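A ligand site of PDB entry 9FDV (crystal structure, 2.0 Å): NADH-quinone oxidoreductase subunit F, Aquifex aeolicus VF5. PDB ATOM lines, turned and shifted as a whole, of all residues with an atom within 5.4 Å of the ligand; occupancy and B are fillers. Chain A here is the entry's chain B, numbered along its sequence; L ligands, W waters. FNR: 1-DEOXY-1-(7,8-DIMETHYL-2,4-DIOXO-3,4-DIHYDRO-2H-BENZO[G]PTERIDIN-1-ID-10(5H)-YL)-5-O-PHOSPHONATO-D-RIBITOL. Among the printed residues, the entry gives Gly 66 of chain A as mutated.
O of Val 218 lies close to O5' of the ligand (3.5 Å). Merely in contact with the ligand: Gly 65, Asp 94, Ser 96, Tyr 180, Ile 181, Glu 184, Gly 394 and Leu 395. Hydrophobic or aromatic side chains that line the ligand: Tyr 180, Ile 181, Val 218 and Leu 395. 19 residues have an atom within 4 Å of the ligand: Gly 65, Gly 66, Gly 67, Lys 76, Asn 92, Asp 94, Glu 95, Ser 96, Tyr 180, Ile 181, Gly 183, Glu 184, Glu 185, Val 218, Asn 219, Asn 220, Thr 223, Gly 394 and Leu 395. The nearest printed residue that does not touch the ligand is Gly 68 (4.3 Å).
The side-chain amide nitrogen (ND2) of Asn 92 lies within hydrogen-bond range of an oxygen (O4') of the ligand (3.1 Å). The side-chain amide oxygen (OD1) of Asn 220 lies close to an oxygen (O2) of the ligand (2.6 Å). N of Glu 95 lies within hydrogen-bond range of O4 of the ligand. OG1 of Thr 223 is in hydrogen-bond range of O3P of the ligand, at 2.6 Å. An oxygen (O2P) of the ligand lies within hydrogen-bond range of the backbone NH of Gly 67 (2.8 Å). N of Asn 220 lies within hydrogen-bond range of O3P of the ligand (2.9 Å). O of Gly 67 is in hydrogen-bond range of N1 of the ligand, 3.4 Å away. N5 of the ligand sits close to O of Gly 183, at 3.5 Å. The side-chain amino group of Lys 76 lies within salt-bridge range of an oxygen (O1P) of the ligand. The side-chain amide oxygen of Asn 219 lies close to an oxygen (O3P) of the ligand, 2.9 Å away. O2' of the ligand lies within hydrogen-bond range of N of Glu 185. An oxygen (O2P) of the ligand lies within hydrogen-bond range of the backbone NH of Gly 66 (3.4 Å).
Water W7 bridges O1P of the ligand (2.6 Å) and N of Phe 71 (2.9 Å). Water W2 lies within hydrogen-bond range of an oxygen (O4) of the ligand (2.6 Å), the backbone NH of Ser 96 (2.8 Å) and the backbone NH of Glu 97 (3.0 Å). Water W6 lies within hydrogen-bond range of O2P of the ligand (2.6 Å), N of Ala 69 (2.9 Å) and N of Gly 68 (3.3 Å). Water W3 lies within hydrogen-bond range of the side-chain hydroxyl of Thr 73 (2.7 Å), an oxygen (O1P) of the ligand (2.8 Å), the backbone carbonyl oxygen of Phe 71 (2.8 Å), the side-chain amide oxygen of Asn 219 (3.4 Å) and the backbone NH of Gly 65 (3.4 Å).
The side-chain carboxylate (OD2) of Asp 103 lies close to the side-chain amide oxygen (OD1) of Asn 220, at 2.9 Å. The backbone carbonyl oxygen (O) of Asn 92 is in hydrogen-bond range of the backbone NH (N) of Val 221. The side-chain amide nitrogen of Asn 92 is in hydrogen-bond range of the backbone carbonyl oxygen of Gly 183, 2.8 Å away. OG1 of Thr 223 lies within hydrogen-bond range of N of Gly 66 (2.9 Å). The backbone NH (N) of Asn 92 is in hydrogen-bond range of the backbone carbonyl oxygen (O) of Asn 219. The side-chain amide oxygen of Asn 92 lies within hydrogen-bond range of the backbone NH of Asp 94, 3.0 Å away. N of Gly 65 lies within hydrogen-bond range of O of Phe 71 (2.9 Å). The backbone NH (N) of Leu 395 lies close to the side-chain sulfur (SG) of Cys 393.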
ATOM      1  N   GLY A  65       1.796  26.749  -9.116  1.00  0.00           N
ATOM      2  CA  GLY A  65       1.852  25.347  -9.535  1.00  0.00           C
ATOM      3  C   GLY A  65       0.756  24.995 -10.548  1.00  0.00           C
ATOM      4  O   GLY A  65      -0.382  25.444 -10.426  1.00  0.00           O
ATOM      5  N   GLY A  66       1.093  24.138 -11.511  1.00  0.00           N
ATOM      6  CA  GLY A  66       0.137  23.700 -12.522  1.00  0.00           C
ATOM      7  C   GLY A  66      -0.444  22.319 -12.211  1.00  0.00           C
ATOM      8  O   GLY A  66      -1.132  21.747 -13.050  1.00  0.00           O
ATOM      9  N   GLY A  67      -0.203  21.787 -11.009  1.00  0.00           N
ATOM     10  CA  GLY A  67      -0.664  20.457 -10.683  1.00  0.00           C
ATOM     11  C   GLY A  67      -2.027  20.425  -9.994  1.00  0.00           C
ATOM     12  O   GLY A  67      -2.495  19.365  -9.614  1.00  0.00           O
ATOM     13  N   GLY A  68      -2.666  21.589  -9.813  1.00  0.00           N
ATOM     14  CA  GLY A  68      -4.053  21.613  -9.371  1.00  0.00           C
ATOM     15  C   GLY A  68      -4.288  22.574  -8.208  1.00  0.00           C
ATOM     16  O   GLY A  68      -5.371  23.146  -8.117  1.00  0.00           O
ATOM     17  N   ALA A  69      -3.293  22.761  -7.341  1.00  0.00           N
ATOM     18  CA  ALA A  69      -3.484  23.555  -6.140  1.00  0.00           C
ATOM     19  C   ALA A  69      -3.120  25.025  -6.363  1.00  0.00           C
ATOM     20  O   ALA A  69      -3.534  25.867  -5.580  1.00  0.00           O
ATOM     21  CB  ALA A  69      -2.713  22.956  -4.978  1.00  0.00           C
ATOM     22  N   GLY A  70      -2.334  25.328  -7.406  1.00  0.00           N
ATOM     23  CA  GLY A  70      -1.971  26.712  -7.687  1.00  0.00           C
ATOM     24  C   GLY A  70      -1.122  27.354  -6.593  1.00  0.00           C
ATOM     25  O   GLY A  70      -1.169  28.561  -6.381  1.00  0.00           O
ATOM     26  N   PHE A  71      -0.289  26.544  -5.900  1.00  0.00           N
ATOM     27  CA  PHE A  71       0.516  27.073  -4.813  1.00  0.00           C
ATOM     28  C   PHE A  71       1.667  27.911  -5.392  1.00  0.00           C
ATOM     29  O   PHE A  71       2.295  27.500  -6.363  1.00  0.00           O
ATOM     30  CB  PHE A  71       1.061  25.955  -3.924  1.00  0.00           C
ATOM     31  CG  PHE A  71       1.607  26.536  -2.625  1.00  0.00           C
ATOM     32  CD1 PHE A  71       0.764  26.790  -1.555  1.00  0.00           C
ATOM     33  CD2 PHE A  71       2.959  26.872  -2.508  1.00  0.00           C
ATOM     34  CE1 PHE A  71       1.252  27.331  -0.373  1.00  0.00           C
ATOM     35  CE2 PHE A  71       3.447  27.413  -1.326  1.00  0.00           C
ATOM     36  CZ  PHE A  71       2.600  27.649  -0.269  1.00  0.00           C
ATOM     37  N   THR A  73       5.118  29.060  -6.460  1.00  0.00           N
ATOM     38  CA  THR A  73       6.241  28.159  -6.584  1.00  0.00           C
ATOM     39  C   THR A  73       7.423  28.666  -5.766  1.00  0.00           C
ATOM     40  O   THR A  73       8.054  27.876  -5.050  1.00  0.00           O
ATOM     41  CB  THR A  73       6.582  27.991  -8.057  1.00  0.00           C
ATOM     42  OG1 THR A  73       5.403  27.465  -8.669  1.00  0.00           O
ATOM     43  CG2 THR A  73       7.777  27.078  -8.280  1.00  0.00           C
ATOM     44  N   LYS A  76       7.128  27.983  -2.110  1.00  0.00           N
ATOM     45  CA  LYS A  76       7.402  26.572  -1.817  1.00  0.00           C
ATOM     46  C   LYS A  76       8.909  26.312  -1.732  1.00  0.00           C
ATOM     47  O   LYS A  76       9.385  25.673  -0.780  1.00  0.00           O
ATOM     48  CB  LYS A  76       6.760  25.681  -2.869  1.00  0.00           C
ATOM     49  CG  LYS A  76       6.850  24.198  -2.562  1.00  0.00           C
ATOM     50  CD  LYS A  76       6.493  23.287  -3.735  1.00  0.00           C
ATOM     51  CE  LYS A  76       5.124  23.472  -4.313  1.00  0.00           C
ATOM     52  NZ  LYS A  76       4.682  22.297  -5.065  1.00  0.00           N
ATOM     53  N   ASN A  92       6.697  16.015 -10.989  1.00  0.00           N
ATOM     54  CA  ASN A  92       5.483  15.225 -11.014  1.00  0.00           C
ATOM     55  C   ASN A  92       4.922  15.147 -12.432  1.00  0.00           C
ATOM     56  O   ASN A  92       4.258  16.071 -12.902  1.00  0.00           O
ATOM     57  CB  ASN A  92       4.473  15.774 -10.011  1.00  0.00           C
ATOM     58  CG  ASN A  92       3.318  14.827  -9.752  1.00  0.00           C
ATOM     59  OD1 ASN A  92       2.980  13.990 -10.593  1.00  0.00           O
ATOM     60  ND2 ASN A  92       2.655  15.029  -8.633  1.00  0.00           N
ATOM     61  N   ASP A  94       2.797  12.519 -13.241  1.00  0.00           N
ATOM     62  CA  ASP A  94       1.829  11.446 -13.059  1.00  0.00           C
ATOM     63  C   ASP A  94       0.510  11.675 -13.793  1.00  0.00           C
ATOM     64  O   ASP A  94      -0.237  10.718 -13.951  1.00  0.00           O
ATOM     65  CB  ASP A  94       1.504  11.131 -11.601  1.00  0.00           C
ATOM     66  CG  ASP A  94       0.944   9.723 -11.459  1.00  0.00           C
ATOM     67  OD1 ASP A  94       1.691   8.800 -11.831  1.00  0.00           O
ATOM     68  OD2 ASP A  94      -0.257   9.569 -11.035  1.00  0.00           O
ATOM     69  N   GLU A  95       0.244  12.923 -14.218  1.00  0.00           N
ATOM     70  CA  GLU A  95      -0.934  13.362 -14.967  1.00  0.00           C
ATOM     71  C   GLU A  95      -1.927  12.234 -15.299  1.00  0.00           C
ATOM     72  O   GLU A  95      -1.849  11.623 -16.353  1.00  0.00           O
ATOM     73  CB  GLU A  95      -0.429  14.026 -16.255  1.00  0.00           C
ATOM     74  CG  GLU A  95      -1.543  14.480 -17.185  1.00  0.00           C
ATOM     75  CD  GLU A  95      -1.094  15.450 -18.261  1.00  0.00           C
ATOM     76  OE1 GLU A  95      -0.523  14.953 -19.256  1.00  0.00           O
ATOM     77  OE2 GLU A  95      -1.340  16.673 -18.107  1.00  0.00           O
ATOM     78  N   SER A  96      -2.906  12.011 -14.417  1.00  0.00           N
ATOM     79  CA  SER A  96      -3.890  10.947 -14.592  1.00  0.00           C
ATOM     80  C   SER A  96      -5.328  11.400 -14.327  1.00  0.00           C
ATOM     81  O   SER A  96      -6.244  10.569 -14.303  1.00  0.00           O
ATOM     82  CB  SER A  96      -3.554   9.793 -13.707  1.00  0.00           C
ATOM     83  OG  SER A  96      -2.388   9.135 -14.184  1.00  0.00           O
ATOM     84  N   GLU A  97      -5.547  12.697 -14.121  1.00  0.00           N
ATOM     85  CA  GLU A  97      -6.902  13.159 -13.894  1.00  0.00           C
ATOM     86  C   GLU A  97      -7.674  13.179 -15.215  1.00  0.00           C
ATOM     87  O   GLU A  97      -7.139  13.640 -16.213  1.00  0.00           O
ATOM     88  CB  GLU A  97      -6.938  14.541 -13.259  1.00  0.00           C
ATOM     89  CG  GLU A  97      -8.312  14.761 -12.624  1.00  0.00           C
ATOM     90  CD  GLU A  97      -8.567  16.143 -12.071  1.00  0.00           C
ATOM     91  OE1 GLU A  97      -7.590  16.928 -11.966  1.00  0.00           O
ATOM     92  OE2 GLU A  97      -9.740  16.408 -11.782  1.00  0.00           O
ATOM     93  N   ASP A 103       0.458  17.966 -19.768  1.00  0.00           N
ATOM     94  CA  ASP A 103       1.849  17.752 -19.399  1.00  0.00           C
ATOM     95  C   ASP A 103       2.566  16.888 -20.428  1.00  0.00           C
ATOM     96  O   ASP A 103       3.743  17.139 -20.734  1.00  0.00           O
ATOM     97  CB  ASP A 103       1.977  17.132 -18.014  1.00  0.00           C
ATOM     98  CG  ASP A 103       1.471  17.990 -16.871  1.00  0.00           C
ATOM     99  OD1 ASP A 103       1.319  19.211 -17.080  1.00  0.00           O
ATOM    100  OD2 ASP A 103       1.188  17.426 -15.771  1.00  0.00           O
ATOM    101  N   TYR A 180      -3.838   6.551  -9.826  1.00  0.00           N
ATOM    102  CA  TYR A 180      -4.008   7.996  -9.869  1.00  0.00           C
ATOM    103  C   TYR A 180      -3.483   8.663  -8.593  1.00  0.00           C
ATOM    104  O   TYR A 180      -3.042   9.807  -8.621  1.00  0.00           O
ATOM    105  CB  TYR A 180      -5.495   8.328 -10.042  1.00  0.00           C
ATOM    106  CG  TYR A 180      -5.902   9.763  -9.737  1.00  0.00           C
ATOM    107  CD1 TYR A 180      -5.504  10.809 -10.577  1.00  0.00           C
ATOM    108  CD2 TYR A 180      -6.724  10.067  -8.662  1.00  0.00           C
ATOM    109  CE1 TYR A 180      -5.871  12.119 -10.319  1.00  0.00           C
ATOM    110  CE2 TYR A 180      -7.122  11.372  -8.412  1.00  0.00           C
ATOM    111  CZ  TYR A 180      -6.693  12.400  -9.245  1.00  0.00           C
ATOM    112  OH  TYR A 180      -7.067  13.678  -8.997  1.00  0.00           O
ATOM    113  N   ILE A 181      -3.575   7.941  -7.481  1.00  0.00           N
ATOM    114  CA  ILE A 181      -3.236   8.499  -6.190  1.00  0.00           C
ATOM    115  C   ILE A 181      -1.740   8.818  -6.116  1.00  0.00           C
ATOM    116  O   ILE A 181      -1.337   9.664  -5.325  1.00  0.00           O
ATOM    117  CB  ILE A 181      -3.687   7.593  -5.032  1.00  0.00           C
ATOM    118  CG1 ILE A 181      -3.615   8.278  -3.687  1.00  0.00           C
ATOM    119  CG2 ILE A 181      -2.882   6.296  -5.009  1.00  0.00           C
ATOM    120  CD1 ILE A 181      -4.368   9.593  -3.624  1.00  0.00           C
ATOM    121  N   GLY A 183      -0.088  10.576  -7.989  1.00  0.00           N
ATOM    122  CA  GLY A 183       0.128  11.975  -8.297  1.00  0.00           C
ATOM    123  C   GLY A 183       0.064  12.878  -7.053  1.00  0.00           C
ATOM    124  O   GLY A 183       0.560  14.010  -7.095  1.00  0.00           O
ATOM    125  N   GLU A 184      -0.544  12.379  -5.976  1.00  0.00           N
ATOM    126  CA  GLU A 184      -0.563  13.089  -4.711  1.00  0.00           C
ATOM    127  C   GLU A 184       0.867  13.069  -4.174  1.00  0.00           C
ATOM    128  O   GLU A 184       1.482  12.013  -4.122  1.00  0.00           O
ATOM    129  CB  GLU A 184      -1.561  12.440  -3.748  1.00  0.00           C
ATOM    130  CG  GLU A 184      -1.945  13.320  -2.555  1.00  0.00           C
ATOM    131  CD  GLU A 184      -1.001  13.297  -1.360  1.00  0.00           C
ATOM    132  OE1 GLU A 184      -0.066  12.463  -1.311  1.00  0.00           O
ATOM    133  OE2 GLU A 184      -1.240  14.103  -0.424  1.00  0.00           O
ATOM    134  N   GLU A 185       1.400  14.235  -3.818  1.00  0.00           N
ATOM    135  CA  GLU A 185       2.849  14.404  -3.631  1.00  0.00           C
ATOM    136  C   GLU A 185       3.431  13.466  -2.571  1.00  0.00           C
ATOM    137  O   GLU A 185       4.552  13.001  -2.741  1.00  0.00           O
ATOM    138  CB  GLU A 185       3.230  15.869  -3.386  1.00  0.00           C
ATOM    139  CG  GLU A 185       2.673  16.439  -2.088  1.00  0.00           C
ATOM    140  CD  GLU A 185       3.070  17.884  -1.793  1.00  0.00           C
ATOM    141  OE1 GLU A 185       3.942  18.445  -2.514  1.00  0.00           O
ATOM    142  OE2 GLU A 185       2.477  18.440  -0.839  1.00  0.00           O
ATOM    143  N   VAL A 218       8.336  18.950  -4.689  1.00  0.00           N
ATOM    144  CA  VAL A 218       7.597  18.309  -5.769  1.00  0.00           C
ATOM    145  C   VAL A 218       6.946  19.417  -6.582  1.00  0.00           C
ATOM    146  O   VAL A 218       6.240  20.255  -6.011  1.00  0.00           O
ATOM    147  CB  VAL A 218       6.515  17.334  -5.267  1.00  0.00           C
ATOM    148  CG1 VAL A 218       5.763  16.692  -6.423  1.00  0.00           C
ATOM    149  CG2 VAL A 218       7.069  16.280  -4.315  1.00  0.00           C
ATOM    150  N   ASN A 219       7.206  19.440  -7.882  1.00  0.00           N
ATOM    151  CA  ASN A 219       6.549  20.382  -8.784  1.00  0.00           C
ATOM    152  C   ASN A 219       6.021  19.659 -10.018  1.00  0.00           C
ATOM    153  O   ASN A 219       6.634  18.703 -10.496  1.00  0.00           O
ATOM    154  CB  ASN A 219       7.476  21.509  -9.240  1.00  0.00           C
ATOM    155  CG  ASN A 219       7.434  22.687  -8.311  1.00  0.00           C
ATOM    156  OD1 ASN A 219       6.359  23.217  -7.987  1.00  0.00           O
ATOM    157  ND2 ASN A 219       8.586  23.063  -7.830  1.00  0.00           N
ATOM    158  N   ASN A 220       4.915  20.169 -10.540  1.00  0.00           N
ATOM    159  CA  ASN A 220       4.316  19.678 -11.771  1.00  0.00           C
ATOM    160  C   ASN A 220       5.168  20.032 -12.996  1.00  0.00           C
ATOM    161  O   ASN A 220       5.848  21.046 -13.017  1.00  0.00           O
ATOM    162  CB  ASN A 220       2.885  20.215 -11.839  1.00  0.00           C
ATOM    163  CG  ASN A 220       2.186  19.777 -13.096  1.00  0.00           C
ATOM    164  OD1 ASN A 220       1.754  18.628 -13.216  1.00  0.00           O
ATOM    165  ND2 ASN A 220       2.101  20.706 -14.030  1.00  0.00           N
ATOM    166  N   VAL A 221       5.094  19.197 -14.037  1.00  0.00           N
ATOM    167  CA  VAL A 221       5.776  19.367 -15.315  1.00  0.00           C
ATOM    168  C   VAL A 221       5.620  20.784 -15.857  1.00  0.00           C
ATOM    169  O   VAL A 221       6.616  21.403 -16.245  1.00  0.00           O
ATOM    170  CB  VAL A 221       5.252  18.352 -16.350  1.00  0.00           C
ATOM    171  CG1 VAL A 221       5.649  18.752 -17.773  1.00  0.00           C
ATOM    172  CG2 VAL A 221       5.720  16.936 -16.048  1.00  0.00           C
ATOM    173  N   THR A 223       4.723  23.579 -14.293  1.00  0.00           N
ATOM    174  CA  THR A 223       5.373  24.551 -13.425  1.00  0.00           C
ATOM    175  C   THR A 223       6.863  24.655 -13.784  1.00  0.00           C
ATOM    176  O   THR A 223       7.384  25.761 -13.924  1.00  0.00           O
ATOM    177  CB  THR A 223       5.251  24.150 -11.954  1.00  0.00           C
ATOM    178  OG1 THR A 223       3.920  23.685 -11.725  1.00  0.00           O
ATOM    179  CG2 THR A 223       5.645  25.284 -11.028  1.00  0.00           C
ATOM    180  N   CYS A 393      -5.965  13.080   2.471  1.00  0.00           N
ATOM    181  CA  CYS A 393      -5.493  13.661   1.216  1.00  0.00           C
ATOM    182  C   CYS A 393      -6.671  14.280   0.452  1.00  0.00           C
ATOM    183  O   CYS A 393      -7.828  14.122   0.860  1.00  0.00           O
ATOM    184  CB  CYS A 393      -4.666  12.672   0.389  1.00  0.00           C
ATOM    185  SG  CYS A 393      -5.582  11.742  -0.887  1.00  0.00           S
ATOM    186  N   GLY A 394      -6.343  14.970  -0.643  1.00  0.00           N
ATOM    187  CA  GLY A 394      -7.306  15.746  -1.412  1.00  0.00           C
ATOM    188  C   GLY A 394      -8.370  14.909  -2.121  1.00  0.00           C
ATOM    189  O   GLY A 394      -9.428  15.433  -2.454  1.00  0.00           O
ATOM    190  N   LEU A 395      -8.115  13.619  -2.367  1.00  0.00           N
ATOM    191  CA  LEU A 395      -9.030  12.793  -3.126  1.00  0.00           C
ATOM    192  C   LEU A 395     -10.336  12.626  -2.342  1.00  0.00           C
ATOM    193  O   LEU A 395     -11.418  12.785  -2.909  1.00  0.00           O
ATOM    194  CB  LEU A 395      -8.425  11.433  -3.446  1.00  0.00           C
ATOM    195  CG  LEU A 395      -9.233  10.538  -4.401  1.00  0.00           C
ATOM    196  CD1 LEU A 395      -8.310   9.660  -5.230  1.00  0.00           C
ATOM    197  CD2 LEU A 395     -10.266   9.673  -3.672  1.00  0.00           C
HETATM  198  C9A FNR L   1      -2.500  15.584  -7.074  1.00  0.00           C
HETATM  199  N10 FNR L   1      -1.519  16.477  -7.585  1.00  0.00           N
HETATM  200  CAA FNR L   1      -0.968  16.235  -8.829  1.00  0.00           C
HETATM  201  N1  FNR L   1       0.029  17.054  -9.272  1.00  0.00           N
HETATM  202  C2  FNR L   1       0.701  16.846 -10.444  1.00  0.00           C
HETATM  203  O2  FNR L   1       1.644  17.560 -10.801  1.00  0.00           O
HETATM  204  N3  FNR L   1       0.270  15.787 -11.194  1.00  0.00           N
HETATM  205  C4  FNR L   1      -0.736  14.898 -10.871  1.00  0.00           C
HETATM  206  O4  FNR L   1      -1.036  14.001 -11.660  1.00  0.00           O
HETATM  207  C4A FNR L   1      -1.341  15.156  -9.596  1.00  0.00           C
HETATM  208  N5  FNR L   1      -2.269  14.292  -9.113  1.00  0.00           N
HETATM  209  C5A FNR L   1      -2.835  14.461  -7.847  1.00  0.00           C
HETATM  210  C6  FNR L   1      -3.753  13.530  -7.362  1.00  0.00           C
HETATM  211  C7  FNR L   1      -4.362  13.722  -6.120  1.00  0.00           C
HETATM  212  C7M FNR L   1      -5.368  12.713  -5.647  1.00  0.00           C
HETATM  213  C8  FNR L   1      -4.034  14.858  -5.356  1.00  0.00           C
HETATM  214  C8M FNR L   1      -4.777  15.180  -4.084  1.00  0.00           C
HETATM  215  C9  FNR L   1      -3.102  15.772  -5.844  1.00  0.00           C
HETATM  216  C1' FNR L   1      -1.074  17.638  -6.800  1.00  0.00           C
HETATM  217  C2' FNR L   1       0.240  17.284  -6.098  1.00  0.00           C
HETATM  218  O2' FNR L   1      -0.010  16.667  -4.824  1.00  0.00           O
HETATM  219  C3' FNR L   1       1.069  18.548  -5.859  1.00  0.00           C
HETATM  220  O3' FNR L   1       0.243  19.583  -5.338  1.00  0.00           O
HETATM  221  C4' FNR L   1       1.802  19.048  -7.100  1.00  0.00           C
HETATM  222  O4' FNR L   1       2.431  17.973  -7.797  1.00  0.00           O
HETATM  223  C5' FNR L   1       2.801  20.121  -6.721  1.00  0.00           C
HETATM  224  O5' FNR L   1       3.361  20.752  -7.887  1.00  0.00           O
HETATM  225  P   FNR L   1       2.864  22.249  -8.276  1.00  0.00           P
HETATM  226  O1P FNR L   1       2.954  23.198  -7.107  1.00  0.00           O
HETATM  227  O2P FNR L   1       1.469  22.153  -8.815  1.00  0.00           O
HETATM  228  O3P FNR L   1       3.881  22.564  -9.370  1.00  0.00           O
HETATM  229  O   HOH W   1       1.676  15.638 -13.808  1.00  0.00           O
HETATM  230  O   HOH W   2      -3.427  14.143 -12.618  1.00  0.00           O
HETATM  231  O   HOH W   3       4.233  25.636  -7.046  1.00  0.00           O
HETATM  232  O   HOH W   4      -1.988  17.844  -3.000  1.00  0.00           O
HETATM  233  O   HOH W   5      -2.156  11.321 -10.876  1.00  0.00           O
HETATM  234  O   HOH W   6      -0.617  21.671  -7.263  1.00  0.00           O
HETATM  235  O   HOH W   7       0.659  23.832  -6.170  1.00  0.00           O
